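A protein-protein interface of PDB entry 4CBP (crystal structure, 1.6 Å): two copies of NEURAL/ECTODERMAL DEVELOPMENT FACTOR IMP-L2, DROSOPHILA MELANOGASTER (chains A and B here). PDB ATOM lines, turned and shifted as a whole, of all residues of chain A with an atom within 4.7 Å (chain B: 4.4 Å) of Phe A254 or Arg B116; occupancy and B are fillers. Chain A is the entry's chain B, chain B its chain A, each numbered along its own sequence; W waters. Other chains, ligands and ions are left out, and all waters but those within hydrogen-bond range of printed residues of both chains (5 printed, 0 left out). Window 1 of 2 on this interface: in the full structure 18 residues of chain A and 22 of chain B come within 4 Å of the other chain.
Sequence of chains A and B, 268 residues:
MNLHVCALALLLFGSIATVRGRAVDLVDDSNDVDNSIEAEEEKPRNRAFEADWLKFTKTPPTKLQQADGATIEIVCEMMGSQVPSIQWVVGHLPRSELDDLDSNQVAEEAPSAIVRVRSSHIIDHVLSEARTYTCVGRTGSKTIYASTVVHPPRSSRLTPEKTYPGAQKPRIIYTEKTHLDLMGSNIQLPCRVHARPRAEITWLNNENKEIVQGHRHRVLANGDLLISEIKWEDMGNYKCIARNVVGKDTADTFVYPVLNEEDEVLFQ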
ATOM      1  N   LYS A 177      -4.324  10.944 -11.029  1.00  0.00           N
ATOM      2  CA  LYS A 177      -4.242   9.938  -9.966  1.00  0.00           C
ATOM      3  C   LYS A 177      -5.299  10.197  -8.890  1.00  0.00           C
ATOM      4  O   LYS A 177      -5.825   9.258  -8.286  1.00  0.00           O
ATOM      5  CB  LYS A 177      -2.849   9.903  -9.348  1.00  0.00           C
ATOM      6  CG  LYS A 177      -1.809   9.249 -10.275  1.00  0.00           C
ATOM      7  CD  LYS A 177      -0.634   8.710  -9.503  1.00  0.00           C
ATOM      8  CE  LYS A 177       0.321   7.971 -10.420  1.00  0.00           C
ATOM      9  NZ  LYS A 177       1.700   7.933  -9.842  1.00  0.00           N
ATOM     10  N   THR A 178      -5.602  11.471  -8.647  1.00  0.00           N
ATOM     11  CA  THR A 178      -6.606  11.838  -7.654  1.00  0.00           C
ATOM     12  C   THR A 178      -7.434  12.990  -8.185  1.00  0.00           C
ATOM     13  O   THR A 178      -6.887  13.948  -8.738  1.00  0.00           O
ATOM     14  CB  THR A 178      -5.967  12.246  -6.296  1.00  0.00           C
ATOM     15  OG1 THR A 178      -5.344  11.107  -5.694  1.00  0.00           O
ATOM     16  CG2 THR A 178      -7.029  12.795  -5.335  1.00  0.00           C
ATOM     17  N   HIS A 179      -8.751  12.883  -8.043  1.00  0.00           N
ATOM     18  CA  HIS A 179      -9.647  13.974  -8.398  1.00  0.00           C
ATOM     19  C   HIS A 179     -10.595  14.241  -7.237  1.00  0.00           C
ATOM     20  O   HIS A 179     -11.576  13.531  -7.029  1.00  0.00           O
ATOM     21  CB  HIS A 179     -10.431  13.657  -9.674  1.00  0.00           C
ATOM     22  CG  HIS A 179     -11.174  14.833 -10.233  1.00  0.00           C
ATOM     23  ND1 HIS A 179     -10.836  15.428 -11.429  1.00  0.00           N
ATOM     24  CD2 HIS A 179     -12.237  15.524  -9.756  1.00  0.00           C
ATOM     25  CE1 HIS A 179     -11.657  16.437 -11.666  1.00  0.00           C
ATOM     26  NE2 HIS A 179     -12.517  16.517 -10.667  1.00  0.00           N
ATOM     27  N   MET A 235     -17.568   7.942  -4.550  1.00  0.00           N
ATOM     28  CA  MET A 235     -16.214   7.948  -4.002  1.00  0.00           C
ATOM     29  C   MET A 235     -15.519   6.617  -4.266  1.00  0.00           C
ATOM     30  O   MET A 235     -16.127   5.550  -4.123  1.00  0.00           O
ATOM     31  CB  MET A 235     -16.239   8.242  -2.495  1.00  0.00           C
ATOM     32  CG  MET A 235     -14.860   8.402  -1.870  1.00  0.00           C
ATOM     33  SD  MET A 235     -14.036   6.709  -1.267  1.00  0.00           S
ATOM     34  CE  MET A 235     -14.838   6.608   0.531  1.00  0.00           C
ATOM     35  N   GLY A 236     -14.248   6.680  -4.664  1.00  0.00           N
ATOM     36  CA  GLY A 236     -13.465   5.475  -4.866  1.00  0.00           C
ATOM     37  C   GLY A 236     -12.604   5.517  -6.109  1.00  0.00           C
ATOM     38  O   GLY A 236     -12.405   6.573  -6.709  1.00  0.00           O
ATOM     39  N   ASN A 237     -12.082   4.352  -6.480  1.00  0.00           N
ATOM     40  CA  ASN A 237     -11.150   4.241  -7.594  1.00  0.00           C
ATOM     41  C   ASN A 237     -11.815   3.845  -8.908  1.00  0.00           C
ATOM     42  O   ASN A 237     -12.650   2.942  -8.947  1.00  0.00           O
ATOM     43  CB  ASN A 237     -10.054   3.232  -7.246  1.00  0.00           C
ATOM     44  CG  ASN A 237      -8.998   3.818  -6.334  1.00  0.00           C
ATOM     45  OD1 ASN A 237      -8.357   4.814  -6.675  1.00  0.00           O
ATOM     46  ND2 ASN A 237      -8.812   3.210  -5.172  1.00  0.00           N
ATOM     47  N   ASP A 252      -5.337   4.025 -12.357  1.00  0.00           N
ATOM     48  CA  ASP A 252      -6.432   4.250 -11.406  1.00  0.00           C
ATOM     49  C   ASP A 252      -6.579   5.726 -11.082  1.00  0.00           C
ATOM     50  O   ASP A 252      -5.584   6.430 -10.869  1.00  0.00           O
ATOM     51  CB  ASP A 252      -6.202   3.492 -10.096  1.00  0.00           C
ATOM     52  CG  ASP A 252      -6.222   1.991 -10.271  1.00  0.00           C
ATOM     53  OD1 ASP A 252      -7.019   1.478 -11.075  1.00  0.00           O
ATOM     54  OD2 ASP A 252      -5.435   1.314  -9.585  1.00  0.00           O
ATOM     55  N   THR A 253      -7.823   6.182 -11.009  1.00  0.00           N
ATOM     56  CA  THR A 253      -8.112   7.548 -10.591  1.00  0.00           C
ATOM     57  C   THR A 253      -8.973   7.524  -9.346  1.00  0.00           C
ATOM     58  O   THR A 253     -10.080   6.974  -9.378  1.00  0.00           O
ATOM     59  CB  THR A 253      -8.843   8.336 -11.691  1.00  0.00           C
ATOM     60  OG1 THR A 253      -8.014   8.409 -12.850  1.00  0.00           O
ATOM     61  CG2 THR A 253      -9.215   9.750 -11.208  1.00  0.00           C
ATOM     62  N   PHE A 254      -8.470   8.096  -8.253  1.00  0.00           N
ATOM     63  CA  PHE A 254      -9.244   8.152  -7.017  1.00  0.00           C
ATOM     64  C   PHE A 254     -10.133   9.396  -6.994  1.00  0.00           C
ATOM     65  O   PHE A 254      -9.634  10.503  -7.127  1.00  0.00           O
ATOM     66  CB  PHE A 254      -8.332   8.156  -5.782  1.00  0.00           C
ATOM     67  CG  PHE A 254      -9.094   8.269  -4.490  1.00  0.00           C
ATOM     68  CD1 PHE A 254      -9.935   7.241  -4.088  1.00  0.00           C
ATOM     69  CD2 PHE A 254      -8.988   9.398  -3.698  1.00  0.00           C
ATOM     70  CE1 PHE A 254     -10.671   7.340  -2.906  1.00  0.00           C
ATOM     71  CE2 PHE A 254      -9.722   9.503  -2.499  1.00  0.00           C
ATOM     72  CZ  PHE A 254     -10.559   8.474  -2.114  1.00  0.00           C
ATOM     73  N   VAL A 255     -11.444   9.193  -6.852  1.00  0.00           N
ATOM     74  CA  VAL A 255     -12.407  10.296  -6.804  1.00  0.00           C
ATOM     75  C   VAL A 255     -12.903  10.506  -5.379  1.00  0.00           C
ATOM     76  O   VAL A 255     -13.360   9.561  -4.728  1.00  0.00           O
ATOM     77  CB  VAL A 255     -13.617  10.032  -7.734  1.00  0.00           C
ATOM     78  CG1 VAL A 255     -14.718  11.110  -7.535  1.00  0.00           C
ATOM     79  CG2 VAL A 255     -13.170   9.944  -9.195  1.00  0.00           C
ATOM     80  N   TYR A 256     -12.803  11.745  -4.897  1.00  0.00           N
ATOM     81  CA  TYR A 256     -13.217  12.078  -3.536  1.00  0.00           C
ATOM     82  C   TYR A 256     -14.171  13.272  -3.546  1.00  0.00           C
ATOM     83  O   TYR A 256     -13.744  14.417  -3.706  1.00  0.00           O
ATOM     84  CB  TYR A 256     -11.994  12.375  -2.650  1.00  0.00           C
ATOM     85  CG  TYR A 256     -12.348  12.471  -1.177  1.00  0.00           C
ATOM     86  CD1 TYR A 256     -12.683  11.331  -0.448  1.00  0.00           C
ATOM     87  CD2 TYR A 256     -12.360  13.694  -0.520  1.00  0.00           C
ATOM     88  CE1 TYR A 256     -13.018  11.406   0.893  1.00  0.00           C
ATOM     89  CE2 TYR A 256     -12.698  13.777   0.832  1.00  0.00           C
ATOM     90  CZ  TYR A 256     -13.029  12.632   1.527  1.00  0.00           C
ATOM     91  OH  TYR A 256     -13.361  12.704   2.867  1.00  0.00           O
ATOM     92  N   THR B  57     -11.666   0.848  -1.098  1.00  0.00           N
ATOM     93  CA  THR B  57     -11.451   1.650  -2.297  1.00  0.00           C
ATOM     94  C   THR B  57     -10.683   0.835  -3.347  1.00  0.00           C
ATOM     95  O   THR B  57     -10.767   1.117  -4.539  1.00  0.00           O
ATOM     96  CB  THR B  57     -10.704   2.952  -1.985  1.00  0.00           C
ATOM     97  OG1 THR B  57      -9.485   2.659  -1.286  1.00  0.00           O
ATOM     98  CG2 THR B  57     -11.570   3.839  -1.114  1.00  0.00           C
ATOM     99  N   GLU B  77      -7.059  -1.704  -0.478  1.00  0.00           N
ATOM    100  CA  GLU B  77      -7.035  -0.306  -0.082  1.00  0.00           C
ATOM    101  C   GLU B  77      -8.394   0.051   0.476  1.00  0.00           C
ATOM    102  O   GLU B  77      -9.413  -0.454   0.005  1.00  0.00           O
ATOM    103  CB  GLU B  77      -6.679   0.592  -1.263  1.00  0.00           C
ATOM    104  CG  GLU B  77      -6.454   2.047  -0.907  1.00  0.00           C
ATOM    105  CD  GLU B  77      -6.297   2.905  -2.140  1.00  0.00           C
ATOM    106  OE1 GLU B  77      -5.156   3.008  -2.629  1.00  0.00           O
ATOM    107  OE2 GLU B  77      -7.317   3.444  -2.640  1.00  0.00           O
ATOM    108  N   MET B  78      -8.402   0.891   1.499  1.00  0.00           N
ATOM    109  CA  MET B  78      -9.649   1.312   2.118  1.00  0.00           C
ATOM    110  C   MET B  78      -9.527   2.726   2.632  1.00  0.00           C
ATOM    111  O   MET B  78      -8.430   3.245   2.820  1.00  0.00           O
ATOM    112  CB  MET B  78     -10.023   0.382   3.271  1.00  0.00           C
ATOM    113  CG  MET B  78      -9.004   0.420   4.375  1.00  0.00           C
ATOM    114  SD  MET B  78      -9.293  -0.979   5.672  1.00  0.00           S
ATOM    115  CE  MET B  78      -9.183  -2.549   4.494  1.00  0.00           C
ATOM    116  N   MET B  79     -10.669   3.356   2.865  1.00  0.00           N
ATOM    117  CA  MET B  79     -10.671   4.683   3.449  1.00  0.00           C
ATOM    118  C   MET B  79     -11.702   4.714   4.557  1.00  0.00           C
ATOM    119  O   MET B  79     -12.767   4.101   4.440  1.00  0.00           O
ATOM    120  CB  MET B  79     -10.988   5.741   2.401  1.00  0.00           C
ATOM    121  CG  MET B  79     -10.760   7.156   2.891  1.00  0.00           C
ATOM    122  SD  MET B  79     -11.115   8.405   1.450  1.00  0.00           S
ATOM    123  CE  MET B  79      -9.902   9.857   1.948  1.00  0.00           C
ATOM    124  N   ILE B 114      -9.548  11.435   8.403  1.00  0.00           N
ATOM    125  CA  ILE B 114     -10.030  10.509   7.393  1.00  0.00           C
ATOM    126  C   ILE B 114      -8.801  10.030   6.637  1.00  0.00           C
ATOM    127  O   ILE B 114      -8.052  10.843   6.112  1.00  0.00           O
ATOM    128  CB  ILE B 114     -11.035  11.155   6.430  1.00  0.00           C
ATOM    129  CG1 ILE B 114     -12.325  11.521   7.181  1.00  0.00           C
ATOM    130  CG2 ILE B 114     -11.368  10.197   5.294  1.00  0.00           C
ATOM    131  CD1 ILE B 114     -13.288  12.359   6.369  1.00  0.00           C
ATOM    132  N   VAL B 115      -8.587   8.719   6.602  1.00  0.00           N
ATOM    133  CA  VAL B 115      -7.349   8.180   6.030  1.00  0.00           C
ATOM    134  C   VAL B 115      -7.636   7.087   5.016  1.00  0.00           C
ATOM    135  O   VAL B 115      -8.455   6.193   5.262  1.00  0.00           O
ATOM    136  CB  VAL B 115      -6.409   7.630   7.137  1.00  0.00           C
ATOM    137  CG1 VAL B 115      -5.236   6.823   6.534  1.00  0.00           C
ATOM    138  CG2 VAL B 115      -5.879   8.774   7.987  1.00  0.00           C
ATOM    139  N   ARG B 116      -6.975   7.191   3.864  1.00  0.00           N
ATOM    140  CA  ARG B 116      -7.005   6.165   2.832  1.00  0.00           C
ATOM    141  C   ARG B 116      -5.680   5.410   2.898  1.00  0.00           C
ATOM    142  O   ARG B 116      -4.610   6.009   2.718  1.00  0.00           O
ATOM    143  CB  ARG B 116      -7.221   6.777   1.440  1.00  0.00           C
ATOM    144  CG  ARG B 116      -7.274   5.736   0.322  1.00  0.00           C
ATOM    145  CD  ARG B 116      -7.808   6.305  -0.992  1.00  0.00           C
ATOM    146  NE  ARG B 116      -6.978   7.344  -1.606  1.00  0.00           N
ATOM    147  CZ  ARG B 116      -6.366   7.230  -2.784  1.00  0.00           C
ATOM    148  NH1 ARG B 116      -6.432   6.097  -3.484  1.00  0.00           N
ATOM    149  NH2 ARG B 116      -5.669   8.252  -3.261  1.00  0.00           N
ATOM    150  N   VAL B 117      -5.761   4.110   3.164  1.00  0.00           N
ATOM    151  CA  VAL B 117      -4.575   3.310   3.447  1.00  0.00           C
ATOM    152  C   VAL B 117      -4.548   2.078   2.547  1.00  0.00           C
ATOM    153  O   VAL B 117      -5.585   1.461   2.283  1.00  0.00           O
ATOM    154  CB  VAL B 117      -4.496   2.913   4.956  1.00  0.00           C
ATOM    155  CG1 VAL B 117      -5.745   2.166   5.407  1.00  0.00           C
ATOM    156  CG2 VAL B 117      -3.230   2.090   5.270  1.00  0.00           C
ATOM    157  N   GLU B 176      -0.016   5.211   3.325  1.00  0.00           N
ATOM    158  CA  GLU B 176      -1.244   5.996   3.286  1.00  0.00           C
ATOM    159  C   GLU B 176      -1.256   6.816   2.002  1.00  0.00           C
ATOM    160  O   GLU B 176      -0.302   7.531   1.713  1.00  0.00           O
ATOM    161  CB  GLU B 176      -1.375   6.908   4.519  1.00  0.00           C
ATOM    162  CG  GLU B 176      -1.731   6.154   5.790  1.00  0.00           C
ATOM    163  CD  GLU B 176      -1.776   7.048   7.023  1.00  0.00           C
ATOM    164  OE1 GLU B 176      -1.619   8.282   6.881  1.00  0.00           O
ATOM    165  OE2 GLU B 176      -1.967   6.513   8.134  1.00  0.00           O
ATOM    166  N   LYS B 177      -2.319   6.672   1.219  1.00  0.00           N
ATOM    167  CA  LYS B 177      -2.515   7.476   0.018  1.00  0.00           C
ATOM    168  C   LYS B 177      -2.966   8.887   0.371  1.00  0.00           C
ATOM    169  O   LYS B 177      -2.541   9.868  -0.238  1.00  0.00           O
ATOM    170  CB  LYS B 177      -3.566   6.837  -0.893  1.00  0.00           C
ATOM    171  CG  LYS B 177      -3.209   5.432  -1.344  1.00  0.00           C
ATOM    172  CD  LYS B 177      -2.050   5.468  -2.275  1.00  0.00           C
ATOM    173  CE  LYS B 177      -2.481   5.807  -3.677  1.00  0.00           C
ATOM    174  NZ  LYS B 177      -1.516   5.208  -4.639  1.00  0.00           N
ATOM    175  N   THR B 178      -3.865   8.966   1.347  1.00  0.00           N
ATOM    176  CA  THR B 178      -4.524  10.223   1.701  1.00  0.00           C
ATOM    177  C   THR B 178      -4.616  10.310   3.209  1.00  0.00           C
ATOM    178  O   THR B 178      -5.088   9.379   3.857  1.00  0.00           O
ATOM    179  CB  THR B 178      -5.945  10.318   1.113  1.00  0.00           C
ATOM    180  OG1 THR B 178      -5.943   9.888  -0.251  1.00  0.00           O
ATOM    181  CG2 THR B 178      -6.480  11.750   1.196  1.00  0.00           C
HETATM  182  O   HOH W   1      -4.342  11.410  -2.932  1.00  0.00           O
HETATM  183  O   HOH W   2      -5.715   5.292  -6.212  1.00  0.00           O
HETATM  184  O   HOH W   3     -11.963  -0.003  -7.387  1.00  0.00           O
HETATM  185  O   HOH W   4     -13.352   2.111  -5.169  1.00  0.00           O
HETATM  186  O   HOH W   5      -4.282   8.545  -5.866  1.00  0.00           O
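Printed residues of chain B within 4 Å of Thr A178: Arg B116 (3.8 Å). Phe A254 touches two residues of chain B. Of the printed residues of chain A, Glu B77 touches Asn A237. Printed residues of chain A within 4 Å of Met B79: Phe A254 (3.6 Å) and Tyr A256 (3.6 Å). Printed residues of chain A within 4 Å of Ile B114: Tyr A256. Arg B116 touches just these residues of chain A: Thr A178 (3.8 Å), Asn A237 (3.9 Å) and Phe A254 (3.4 Å). The nearest residue of chain B that does not touch Phe A254 is Thr B57 (4.03 Å).
The side-chain amide nitrogen (ND2) of Asn A237 lies within hydrogen-bond range of the backbone carbonyl oxygen (O) of Thr B57, 2.9 Å away. The side-chain amide nitrogen of Asn A237 lies within hydrogen-bond range of the side-chain carboxylate of Glu B77, 2.9 Å away.
2 positions are printed for both chains.
The side-chain carboxylate (OE2) of Glu B77 sits at hydrogen-bond distance from the side-chain hydroxyl (OG1) of Thr B57 (2.7 Å). The side-chain hydroxyl (OG1) of Thr B57 is in hydrogen-bond range of the backbone NH (N) of Met B78, at 3.5 Å. The backbone carbonyl oxygen (O) of Arg B116 is in hydrogen-bond range of the backbone NH (N) of Lys B177 (2.8 Å). The backbone carbonyl oxygen (O) of Lys A177 sits at hydrogen-bond distance from the backbone NH (N) of Phe A254 (2.9 Å). N of His A179 lies within hydrogen-bond range of O of Phe A254. The backbone carbonyl oxygen (O) of His A179 is in hydrogen-bond range of the backbone NH (N) of Tyr A256, at 3.0 Å.
Water W2 lies within hydrogen-bond range of OD1 of Asn A237 and NH1 of Arg B116. Water W5 lies within hydrogen-bond range of OG1 of Thr A178 (2.8 Å), O of Lys A177 (3.0 Å) and NH2 of Arg B116 (3.0 Å). Water W4 lies within hydrogen-bond range of O of Thr B57 (2.8 Å) and N of Asn A237 (2.9 Å). Water W1 lies within hydrogen-bond range of the side-chain hydroxyl (OG1) of Thr A178 (3.0 Å), the guanidinium group (NH2) of Arg B116 (3.4 Å) and the side-chain hydroxyl (OG1) of Thr B178 (3.5 Å). Water W3 bridges O of Thr B57 and O of Asn A237.
Hydrophobic or aromatic side chains of chain A that line the printed part of chain B: Met A235, Phe A254 and Tyr A256. Along chain A the printed residues that touch a printed residue of chain B span positions 178 to 256. Of the 11 printed residues of chain B, 5 touch a printed residue of chain A. Hydrophobic or aromatic side chains of chain B that line the printed part of chain A: Met B79 and Ile B114. Among the printed residues, 9 pairs touch across the chains. Among the printed residues, no Asp or Glu carboxylate lies within 4 Å of a Lys or Arg side-chain nitrogen of the other chain.
Among the printed residues, merely in contact across the chains: Thr A178 with Arg B116 (3.8 Å), Met A235 with Thr B57 (3.8 Å), Asn A237 with Arg B116 (3.9 Å), Phe A254 with Met B79 (3.6 Å), Phe A254 with Arg B116 (3.4 Å), Tyr A256 with Met B79 (3.6 Å) and Tyr A256 with Ile B114 (3.5 Å).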
